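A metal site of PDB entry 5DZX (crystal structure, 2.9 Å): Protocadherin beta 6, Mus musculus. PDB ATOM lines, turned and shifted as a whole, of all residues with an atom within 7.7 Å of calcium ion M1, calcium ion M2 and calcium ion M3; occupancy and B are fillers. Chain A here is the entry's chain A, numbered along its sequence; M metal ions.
Calcium ion M2 is bound by OE2 of Glu 9 (2.2 Å).
Calcium ion M2 is bound by the side-chain carboxylate (OD2) of Asp 100.
The side-chain carboxylate (OD1) of Asp 63 is bound to calcium ion M2 (2.5 Å).
The side-chain carboxylate (OE2) of Glu 10 is bound to calcium ion M2, 2.6 Å away.
OE1 of Glu 65 binds calcium ion M2 (2.7 Å).
Calcium ion M2 has five donor atoms within binding distance.
Calcium ion M1 is bound by the side-chain carboxylate of Glu 65 (2.2 Å), the side-chain carboxylate of Glu 9 (2.4 Å), the side-chain carboxylate of Asp 97 (2.4 Å), the side-chain carboxylate of Asp 100 (2.4 Å), the side-chain carboxylate of Asp 133 (2.5 Å) and the backbone carbonyl oxygen of Ile 98 (2.5 Å).
Calcium ion M3 is bound by the backbone carbonyl oxygen of His 101, the side-chain amide oxygen of Asn 99, the backbone carbonyl oxygen of Asn 137, the side-chain carboxylate of Asp 133, the side-chain carboxylate of Asp 188 and the side-chain carboxylate of Asp 131.
Slightly farther from calcium ion M3 lies OD1 of Asp 131 (3.0 Å).
Of the 28 residues printed, 6 come within 4 Å of calcium ion M1.
The nearest printed residue that does not touch calcium ion M1 is His 101 (4.3 Å).
Of the 28 residues printed, 6 come within 4 Å of calcium ion M3.
The backbone NH (N) of Glu 9 is in hydrogen-bond range of the backbone carbonyl oxygen (O) of Thr 96 (2.7 Å).
NH1 of Arg 64 lies close to OE2 of Glu 65 (3.3 Å).
The side-chain carboxylate (OD1) of Asp 100 sits close to a ring nitrogen (ND1) of His 101, 2.9 Å away.
The side-chain amino group (NZ) of Lys 194 lies within hydrogen-bond range of the backbone carbonyl oxygen (O) of Asn 99 (3.2 Å).
The side-chain carboxylate (OD2) of Asp 97 is in salt-bridge range of the guanidinium group (NH2) of Arg 64, at 3.8 Å.
The side-chain carboxylate (OD2) of Asp 97 sits at hydrogen-bond distance from the backbone NH (N) of Ile 134 (3.2 Å).
The backbone NH (N) of Gly 190 sits at hydrogen-bond distance from the side-chain carboxylate (OD1) of Asp 188 (2.9 Å).
O of Pro 62 sits at hydrogen-bond distance from N of Glu 10 (2.7 Å).
Within 4 Å of calcium ion M2: Glu 9, Glu 10, Asp 63, Glu 65, Asp 100 and His 101.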
ATOM      1  N   GLU A   9      14.091 -11.653  -2.966  1.00  0.00           N
ATOM      2  CA  GLU A   9      15.367 -12.292  -2.689  1.00  0.00           C
ATOM      3  C   GLU A   9      15.705 -13.312  -3.766  1.00  0.00           C
ATOM      4  O   GLU A   9      14.811 -13.875  -4.405  1.00  0.00           O
ATOM      5  CB  GLU A   9      15.329 -12.950  -1.310  1.00  0.00           C
ATOM      6  CG  GLU A   9      16.602 -13.658  -0.901  1.00  0.00           C
ATOM      7  CD  GLU A   9      16.344 -14.788   0.064  1.00  0.00           C
ATOM      8  OE1 GLU A   9      15.266 -14.789   0.701  1.00  0.00           O
ATOM      9  OE2 GLU A   9      17.208 -15.679   0.189  1.00  0.00           O
ATOM     10  N   GLU A  10      17.003 -13.528  -3.998  1.00  0.00           N
ATOM     11  CA  GLU A  10      17.500 -14.559  -4.902  1.00  0.00           C
ATOM     12  C   GLU A  10      17.036 -14.357  -6.348  1.00  0.00           C
ATOM     13  O   GLU A  10      16.894 -15.311  -7.101  1.00  0.00           O
ATOM     14  CB  GLU A  10      17.090 -15.956  -4.431  1.00  0.00           C
ATOM     15  CG  GLU A  10      17.561 -16.329  -3.028  1.00  0.00           C
ATOM     16  CD  GLU A  10      19.035 -16.703  -2.974  1.00  0.00           C
ATOM     17  OE1 GLU A  10      19.732 -16.595  -4.002  1.00  0.00           O
ATOM     18  OE2 GLU A  10      19.492 -17.115  -1.886  1.00  0.00           O
ATOM     19  N   PRO A  62      21.011 -11.627  -4.888  1.00  0.00           N
ATOM     20  CA  PRO A  62      20.902 -11.176  -3.493  1.00  0.00           C
ATOM     21  C   PRO A  62      20.319 -12.240  -2.568  1.00  0.00           C
ATOM     22  O   PRO A  62      19.239 -12.757  -2.800  1.00  0.00           O
ATOM     23  CB  PRO A  62      19.947  -9.983  -3.605  1.00  0.00           C
ATOM     24  CG  PRO A  62      19.074 -10.320  -4.764  1.00  0.00           C
ATOM     25  CD  PRO A  62      19.919 -11.117  -5.728  1.00  0.00           C
ATOM     26  N   ASP A  63      21.063 -12.553  -1.507  1.00  0.00           N
ATOM     27  CA  ASP A  63      20.596 -13.496  -0.501  1.00  0.00           C
ATOM     28  C   ASP A  63      20.248 -12.763   0.786  1.00  0.00           C
ATOM     29  O   ASP A  63      21.117 -12.208   1.451  1.00  0.00           O
ATOM     30  CB  ASP A  63      21.647 -14.572  -0.238  1.00  0.00           C
ATOM     31  CG  ASP A  63      21.151 -15.661   0.685  1.00  0.00           C
ATOM     32  OD1 ASP A  63      19.930 -15.917   0.694  1.00  0.00           O
ATOM     33  OD2 ASP A  63      21.980 -16.250   1.420  1.00  0.00           O
ATOM     34  N   ARG A  64      18.956 -12.759   1.125  1.00  0.00           N
ATOM     35  CA  ARG A  64      18.460 -12.045   2.290  1.00  0.00           C
ATOM     36  C   ARG A  64      19.117 -12.548   3.574  1.00  0.00           C
ATOM     37  O   ARG A  64      19.630 -11.754   4.373  1.00  0.00           O
ATOM     38  CB  ARG A  64      16.932 -12.187   2.384  1.00  0.00           C
ATOM     39  CG  ARG A  64      16.206 -10.996   3.009  1.00  0.00           C
ATOM     40  CD  ARG A  64      16.448 -10.875   4.512  1.00  0.00           C
ATOM     41  NE  ARG A  64      16.371 -12.173   5.187  1.00  0.00           N
ATOM     42  CZ  ARG A  64      15.236 -12.741   5.561  1.00  0.00           C
ATOM     43  NH1 ARG A  64      15.245 -13.918   6.179  1.00  0.00           N
ATOM     44  NH2 ARG A  64      14.076 -12.142   5.330  1.00  0.00           N
ATOM     45  N   GLU A  65      19.117 -13.858   3.761  1.00  0.00           N
ATOM     46  CA  GLU A  65      19.598 -14.474   4.993  1.00  0.00           C
ATOM     47  C   GLU A  65      21.098 -14.288   5.215  1.00  0.00           C
ATOM     48  O   GLU A  65      21.609 -14.536   6.303  1.00  0.00           O
ATOM     49  CB  GLU A  65      19.261 -15.965   5.005  1.00  0.00           C
ATOM     50  CG  GLU A  65      17.768 -16.289   5.055  1.00  0.00           C
ATOM     51  CD  GLU A  65      17.091 -16.177   3.703  1.00  0.00           C
ATOM     52  OE1 GLU A  65      17.783 -16.344   2.678  1.00  0.00           O
ATOM     53  OE2 GLU A  65      15.873 -15.920   3.671  1.00  0.00           O
ATOM     54  N   ALA A  66      21.805 -13.848   4.171  1.00  0.00           N
ATOM     55  CA  ALA A  66      23.253 -13.684   4.251  1.00  0.00           C
ATOM     56  C   ALA A  66      23.666 -12.222   4.243  1.00  0.00           C
ATOM     57  O   ALA A  66      24.817 -11.891   4.532  1.00  0.00           O
ATOM     58  CB  ALA A  66      23.927 -14.422   3.100  1.00  0.00           C
ATOM     59  N   THR A  96      12.757  -8.287  -0.679  1.00  0.00           N
ATOM     60  CA  THR A  96      11.601  -9.032  -0.199  1.00  0.00           C
ATOM     61  C   THR A  96      11.980 -10.486   0.057  1.00  0.00           C
ATOM     62  O   THR A  96      12.617 -11.127  -0.785  1.00  0.00           O
ATOM     63  CB  THR A  96      10.425  -8.971  -1.182  1.00  0.00           C
ATOM     64  OG1 THR A  96      10.061  -7.606  -1.424  1.00  0.00           O
ATOM     65  CG2 THR A  96       9.213  -9.705  -0.615  1.00  0.00           C
ATOM     66  N   ASP A  97      11.573 -11.007   1.208  1.00  0.00           N
ATOM     67  CA  ASP A  97      11.886 -12.380   1.584  1.00  0.00           C
ATOM     68  C   ASP A  97      11.038 -13.377   0.808  1.00  0.00           C
ATOM     69  O   ASP A  97       9.811 -13.254   0.752  1.00  0.00           O
ATOM     70  CB  ASP A  97      11.688 -12.588   3.079  1.00  0.00           C
ATOM     71  CG  ASP A  97      12.033 -13.995   3.515  1.00  0.00           C
ATOM     72  OD1 ASP A  97      12.992 -14.569   2.950  1.00  0.00           O
ATOM     73  OD2 ASP A  97      11.333 -14.542   4.390  1.00  0.00           O
ATOM     74  N   ILE A  98      11.690 -14.375   0.236  1.00  0.00           N
ATOM     75  CA  ILE A  98      10.991 -15.441  -0.462  1.00  0.00           C
ATOM     76  C   ILE A  98      11.240 -16.780   0.248  1.00  0.00           C
ATOM     77  O   ILE A  98      12.355 -17.047   0.692  1.00  0.00           O
ATOM     78  CB  ILE A  98      11.430 -15.526  -1.931  1.00  0.00           C
ATOM     79  CG1 ILE A  98      12.955 -15.507  -2.046  1.00  0.00           C
ATOM     80  CG2 ILE A  98      10.843 -14.361  -2.721  1.00  0.00           C
ATOM     81  CD1 ILE A  98      13.572 -16.856  -2.334  1.00  0.00           C
ATOM     82  N   ASN A  99      10.188 -17.587   0.361  1.00  0.00           N
ATOM     83  CA  ASN A  99      10.258 -18.839   1.103  1.00  0.00           C
ATOM     84  C   ASN A  99      11.124 -19.884   0.399  1.00  0.00           C
ATOM     85  O   ASN A  99      10.610 -20.709  -0.355  1.00  0.00           O
ATOM     86  CB  ASN A  99       8.845 -19.390   1.317  1.00  0.00           C
ATOM     87  CG  ASN A  99       8.813 -20.537   2.312  1.00  0.00           C
ATOM     88  OD1 ASN A  99       9.681 -20.650   3.165  1.00  0.00           O
ATOM     89  ND2 ASN A  99       7.803 -21.393   2.195  1.00  0.00           N
ATOM     90  N   ASP A 100      12.418 -19.864   0.674  1.00  0.00           N
ATOM     91  CA  ASP A 100      13.346 -20.784   0.042  1.00  0.00           C
ATOM     92  C   ASP A 100      14.058 -21.661   1.063  1.00  0.00           C
ATOM     93  O   ASP A 100      15.117 -22.224   0.789  1.00  0.00           O
ATOM     94  CB  ASP A 100      14.374 -20.008  -0.808  1.00  0.00           C
ATOM     95  CG  ASP A 100      15.149 -18.982   0.000  1.00  0.00           C
ATOM     96  OD1 ASP A 100      14.688 -18.589   1.097  1.00  0.00           O
ATOM     97  OD2 ASP A 100      16.220 -18.541  -0.469  1.00  0.00           O
ATOM     98  N   HIS A 101      13.460 -21.789   2.241  1.00  0.00           N
ATOM     99  CA  HIS A 101      13.993 -22.650   3.290  1.00  0.00           C
ATOM    100  C   HIS A 101      12.909 -23.497   3.933  1.00  0.00           C
ATOM    101  O   HIS A 101      11.854 -22.987   4.313  1.00  0.00           O
ATOM    102  CB  HIS A 101      14.708 -21.810   4.359  1.00  0.00           C
ATOM    103  CG  HIS A 101      16.026 -21.268   3.913  1.00  0.00           C
ATOM    104  ND1 HIS A 101      16.146 -20.314   2.922  1.00  0.00           N
ATOM    105  CD2 HIS A 101      17.284 -21.556   4.321  1.00  0.00           C
ATOM    106  CE1 HIS A 101      17.422 -20.038   2.745  1.00  0.00           C
ATOM    107  NE2 HIS A 101      18.135 -20.770   3.576  1.00  0.00           N
ATOM    108  N   SER A 102      13.167 -24.793   4.070  1.00  0.00           N
ATOM    109  CA  SER A 102      12.211 -25.695   4.678  1.00  0.00           C
ATOM    110  C   SER A 102      12.444 -25.807   6.185  1.00  0.00           C
ATOM    111  O   SER A 102      13.587 -25.873   6.629  1.00  0.00           O
ATOM    112  CB  SER A 102      12.283 -27.079   4.035  1.00  0.00           C
ATOM    113  OG  SER A 102      12.069 -26.987   2.633  1.00  0.00           O
ATOM    114  N   PRO A 103      11.351 -25.835   6.968  1.00  0.00           N
ATOM    115  CA  PRO A 103      11.452 -26.032   8.414  1.00  0.00           C
ATOM    116  C   PRO A 103      12.228 -27.303   8.724  1.00  0.00           C
ATOM    117  O   PRO A 103      11.964 -28.350   8.146  1.00  0.00           O
ATOM    118  CB  PRO A 103       9.995 -26.160   8.857  1.00  0.00           C
ATOM    119  CG  PRO A 103       9.233 -25.393   7.837  1.00  0.00           C
ATOM    120  CD  PRO A 103       9.954 -25.651   6.539  1.00  0.00           C
ATOM    121  N   GLN A 130      14.076 -24.953  13.303  1.00  0.00           N
ATOM    122  CA  GLN A 130      14.802 -23.780  12.850  1.00  0.00           C
ATOM    123  C   GLN A 130      14.477 -23.444  11.394  1.00  0.00           C
ATOM    124  O   GLN A 130      14.467 -24.313  10.528  1.00  0.00           O
ATOM    125  CB  GLN A 130      16.309 -23.981  13.042  1.00  0.00           C
ATOM    126  CG  GLN A 130      16.824 -25.342  12.599  1.00  0.00           C
ATOM    127  CD  GLN A 130      18.159 -25.682  13.222  1.00  0.00           C
ATOM    128  OE1 GLN A 130      18.649 -24.969  14.093  1.00  0.00           O
ATOM    129  NE2 GLN A 130      18.757 -26.791  12.788  1.00  0.00           N
ATOM    130  N   ASP A 131      14.225 -22.170  11.146  1.00  0.00           N
ATOM    131  CA  ASP A 131      13.934 -21.679   9.803  1.00  0.00           C
ATOM    132  C   ASP A 131      14.671 -20.366   9.554  1.00  0.00           C
ATOM    133  O   ASP A 131      14.619 -19.460  10.381  1.00  0.00           O
ATOM    134  CB  ASP A 131      12.421 -21.491   9.609  1.00  0.00           C
ATOM    135  CG  ASP A 131      12.018 -21.442   8.152  1.00  0.00           C
ATOM    136  OD1 ASP A 131      12.813 -20.933   7.330  1.00  0.00           O
ATOM    137  OD2 ASP A 131      10.913 -21.905   7.820  1.00  0.00           O
ATOM    138  N   SER A 132      15.353 -20.279   8.421  1.00  0.00           N
ATOM    139  CA  SER A 132      16.110 -19.077   8.075  1.00  0.00           C
ATOM    140  C   SER A 132      15.189 -17.939   7.653  1.00  0.00           C
ATOM    141  O   SER A 132      15.488 -16.777   7.900  1.00  0.00           O
ATOM    142  CB  SER A 132      17.108 -19.379   6.954  1.00  0.00           C
ATOM    143  OG  SER A 132      18.089 -20.316   7.375  1.00  0.00           O
ATOM    144  N   ASP A 133      14.066 -18.286   7.032  1.00  0.00           N
ATOM    145  CA  ASP A 133      13.101 -17.288   6.579  1.00  0.00           C
ATOM    146  C   ASP A 133      12.418 -16.597   7.751  1.00  0.00           C
ATOM    147  O   ASP A 133      12.550 -17.025   8.900  1.00  0.00           O
ATOM    148  CB  ASP A 133      12.050 -17.942   5.670  1.00  0.00           C
ATOM    149  CG  ASP A 133      12.659 -18.571   4.436  1.00  0.00           C
ATOM    150  OD1 ASP A 133      13.662 -18.033   3.917  1.00  0.00           O
ATOM    151  OD2 ASP A 133      12.130 -19.610   3.982  1.00  0.00           O
ATOM    152  N   ILE A 134      11.696 -15.521   7.459  1.00  0.00           N
ATOM    153  CA  ILE A 134      11.001 -14.769   8.498  1.00  0.00           C
ATOM    154  C   ILE A 134       9.562 -14.488   8.084  1.00  0.00           C
ATOM    155  O   ILE A 134       9.158 -14.768   6.959  1.00  0.00           O
ATOM    156  CB  ILE A 134      11.722 -13.441   8.825  1.00  0.00           C
ATOM    157  CG1 ILE A 134      11.848 -12.561   7.571  1.00  0.00           C
ATOM    158  CG2 ILE A 134      13.094 -13.698   9.420  1.00  0.00           C
ATOM    159  CD1 ILE A 134      10.821 -11.454   7.465  1.00  0.00           C
ATOM    160  N   SER A 136       5.797 -14.558   7.275  1.00  0.00           N
ATOM    161  CA  SER A 136       4.883 -15.592   6.793  1.00  0.00           C
ATOM    162  C   SER A 136       5.641 -16.792   6.225  1.00  0.00           C
ATOM    163  O   SER A 136       5.083 -17.887   6.113  1.00  0.00           O
ATOM    164  CB  SER A 136       3.943 -15.011   5.731  1.00  0.00           C
ATOM    165  OG  SER A 136       3.071 -15.996   5.215  1.00  0.00           O
ATOM    166  N   ASN A 137       6.894 -16.589   5.855  1.00  0.00           N
ATOM    167  CA  ASN A 137       7.716 -17.651   5.276  1.00  0.00           C
ATOM    168  C   ASN A 137       8.420 -18.499   6.331  1.00  0.00           C
ATOM    169  O   ASN A 137       9.098 -19.472   5.993  1.00  0.00           O
ATOM    170  CB  ASN A 137       8.737 -17.065   4.314  1.00  0.00           C
ATOM    171  CG  ASN A 137       8.103 -16.514   3.053  1.00  0.00           C
ATOM    172  OD1 ASN A 137       7.042 -16.989   2.627  1.00  0.00           O
ATOM    173  ND2 ASN A 137       8.730 -15.513   2.447  1.00  0.00           N
ATOM    174  N   ALA A 138       8.270 -18.123   7.589  1.00  0.00           N
ATOM    175  CA  ALA A 138       8.835 -18.897   8.682  1.00  0.00           C
ATOM    176  C   ALA A 138       7.833 -19.951   9.156  1.00  0.00           C
ATOM    177  O   ALA A 138       6.738 -20.057   8.620  1.00  0.00           O
ATOM    178  CB  ALA A 138       9.241 -17.997   9.834  1.00  0.00           C
ATOM    179  N   VAL A 139       8.223 -20.714  10.168  1.00  0.00           N
ATOM    180  CA  VAL A 139       7.345 -21.707  10.770  1.00  0.00           C
ATOM    181  C   VAL A 139       6.096 -21.015  11.313  1.00  0.00           C
ATOM    182  O   VAL A 139       6.202 -19.989  11.985  1.00  0.00           O
ATOM    183  CB  VAL A 139       8.054 -22.481  11.887  1.00  0.00           C
ATOM    184  CG1 VAL A 139       7.100 -23.455  12.541  1.00  0.00           C
ATOM    185  CG2 VAL A 139       9.264 -23.208  11.330  1.00  0.00           C
ATOM    186  N   ASP A 188       5.085 -24.663   7.557  1.00  0.00           N
ATOM    187  CA  ASP A 188       5.434 -23.332   7.124  1.00  0.00           C
ATOM    188  C   ASP A 188       4.172 -22.557   6.755  1.00  0.00           C
ATOM    189  O   ASP A 188       3.142 -23.143   6.426  1.00  0.00           O
ATOM    190  CB  ASP A 188       6.392 -23.404   5.934  1.00  0.00           C
ATOM    191  CG  ASP A 188       7.167 -22.132   5.722  1.00  0.00           C
ATOM    192  OD1 ASP A 188       6.622 -21.203   5.079  1.00  0.00           O
ATOM    193  OD2 ASP A 188       8.321 -22.056   6.183  1.00  0.00           O
ATOM    194  N   GLY A 189       4.251 -21.225   6.811  1.00  0.00           N
ATOM    195  CA  GLY A 189       3.108 -20.390   6.499  1.00  0.00           C
ATOM    196  C   GLY A 189       2.970 -20.051   5.025  1.00  0.00           C
ATOM    197  O   GLY A 189       1.912 -19.612   4.575  1.00  0.00           O
ATOM    198  N   GLY A 190       4.045 -20.258   4.274  1.00  0.00           N
ATOM    199  CA  GLY A 190       4.066 -19.942   2.857  1.00  0.00           C
ATOM    200  C   GLY A 190       3.135 -20.801   2.024  1.00  0.00           C
ATOM    201  O   GLY A 190       2.588 -21.802   2.502  1.00  0.00           O
ATOM    202  N   LYS A 194       5.889 -25.749   3.595  1.00  0.00           N
ATOM    203  CA  LYS A 194       6.975 -26.738   3.593  1.00  0.00           C
ATOM    204  C   LYS A 194       7.017 -27.503   4.913  1.00  0.00           C
ATOM    205  O   LYS A 194       6.816 -26.928   5.989  1.00  0.00           O
ATOM    206  CB  LYS A 194       8.323 -26.059   3.321  1.00  0.00           C
ATOM    207  CG  LYS A 194       8.421 -25.459   1.933  1.00  0.00           C
ATOM    208  CD  LYS A 194       9.790 -24.854   1.663  1.00  0.00           C
ATOM    209  CE  LYS A 194       9.892 -24.358   0.229  1.00  0.00           C
ATOM    210  NZ  LYS A 194      11.235 -23.826  -0.097  1.00  0.00           N
HETATM  211 CA    CA M   1      14.322 -16.438   2.172  1.00  0.00          CA
HETATM  212 CA    CA M   2      18.171 -17.599   0.349  1.00  0.00          CA
HETATM  213 CA    CA M   3      10.648 -21.300   5.249  1.00  0.00          CA
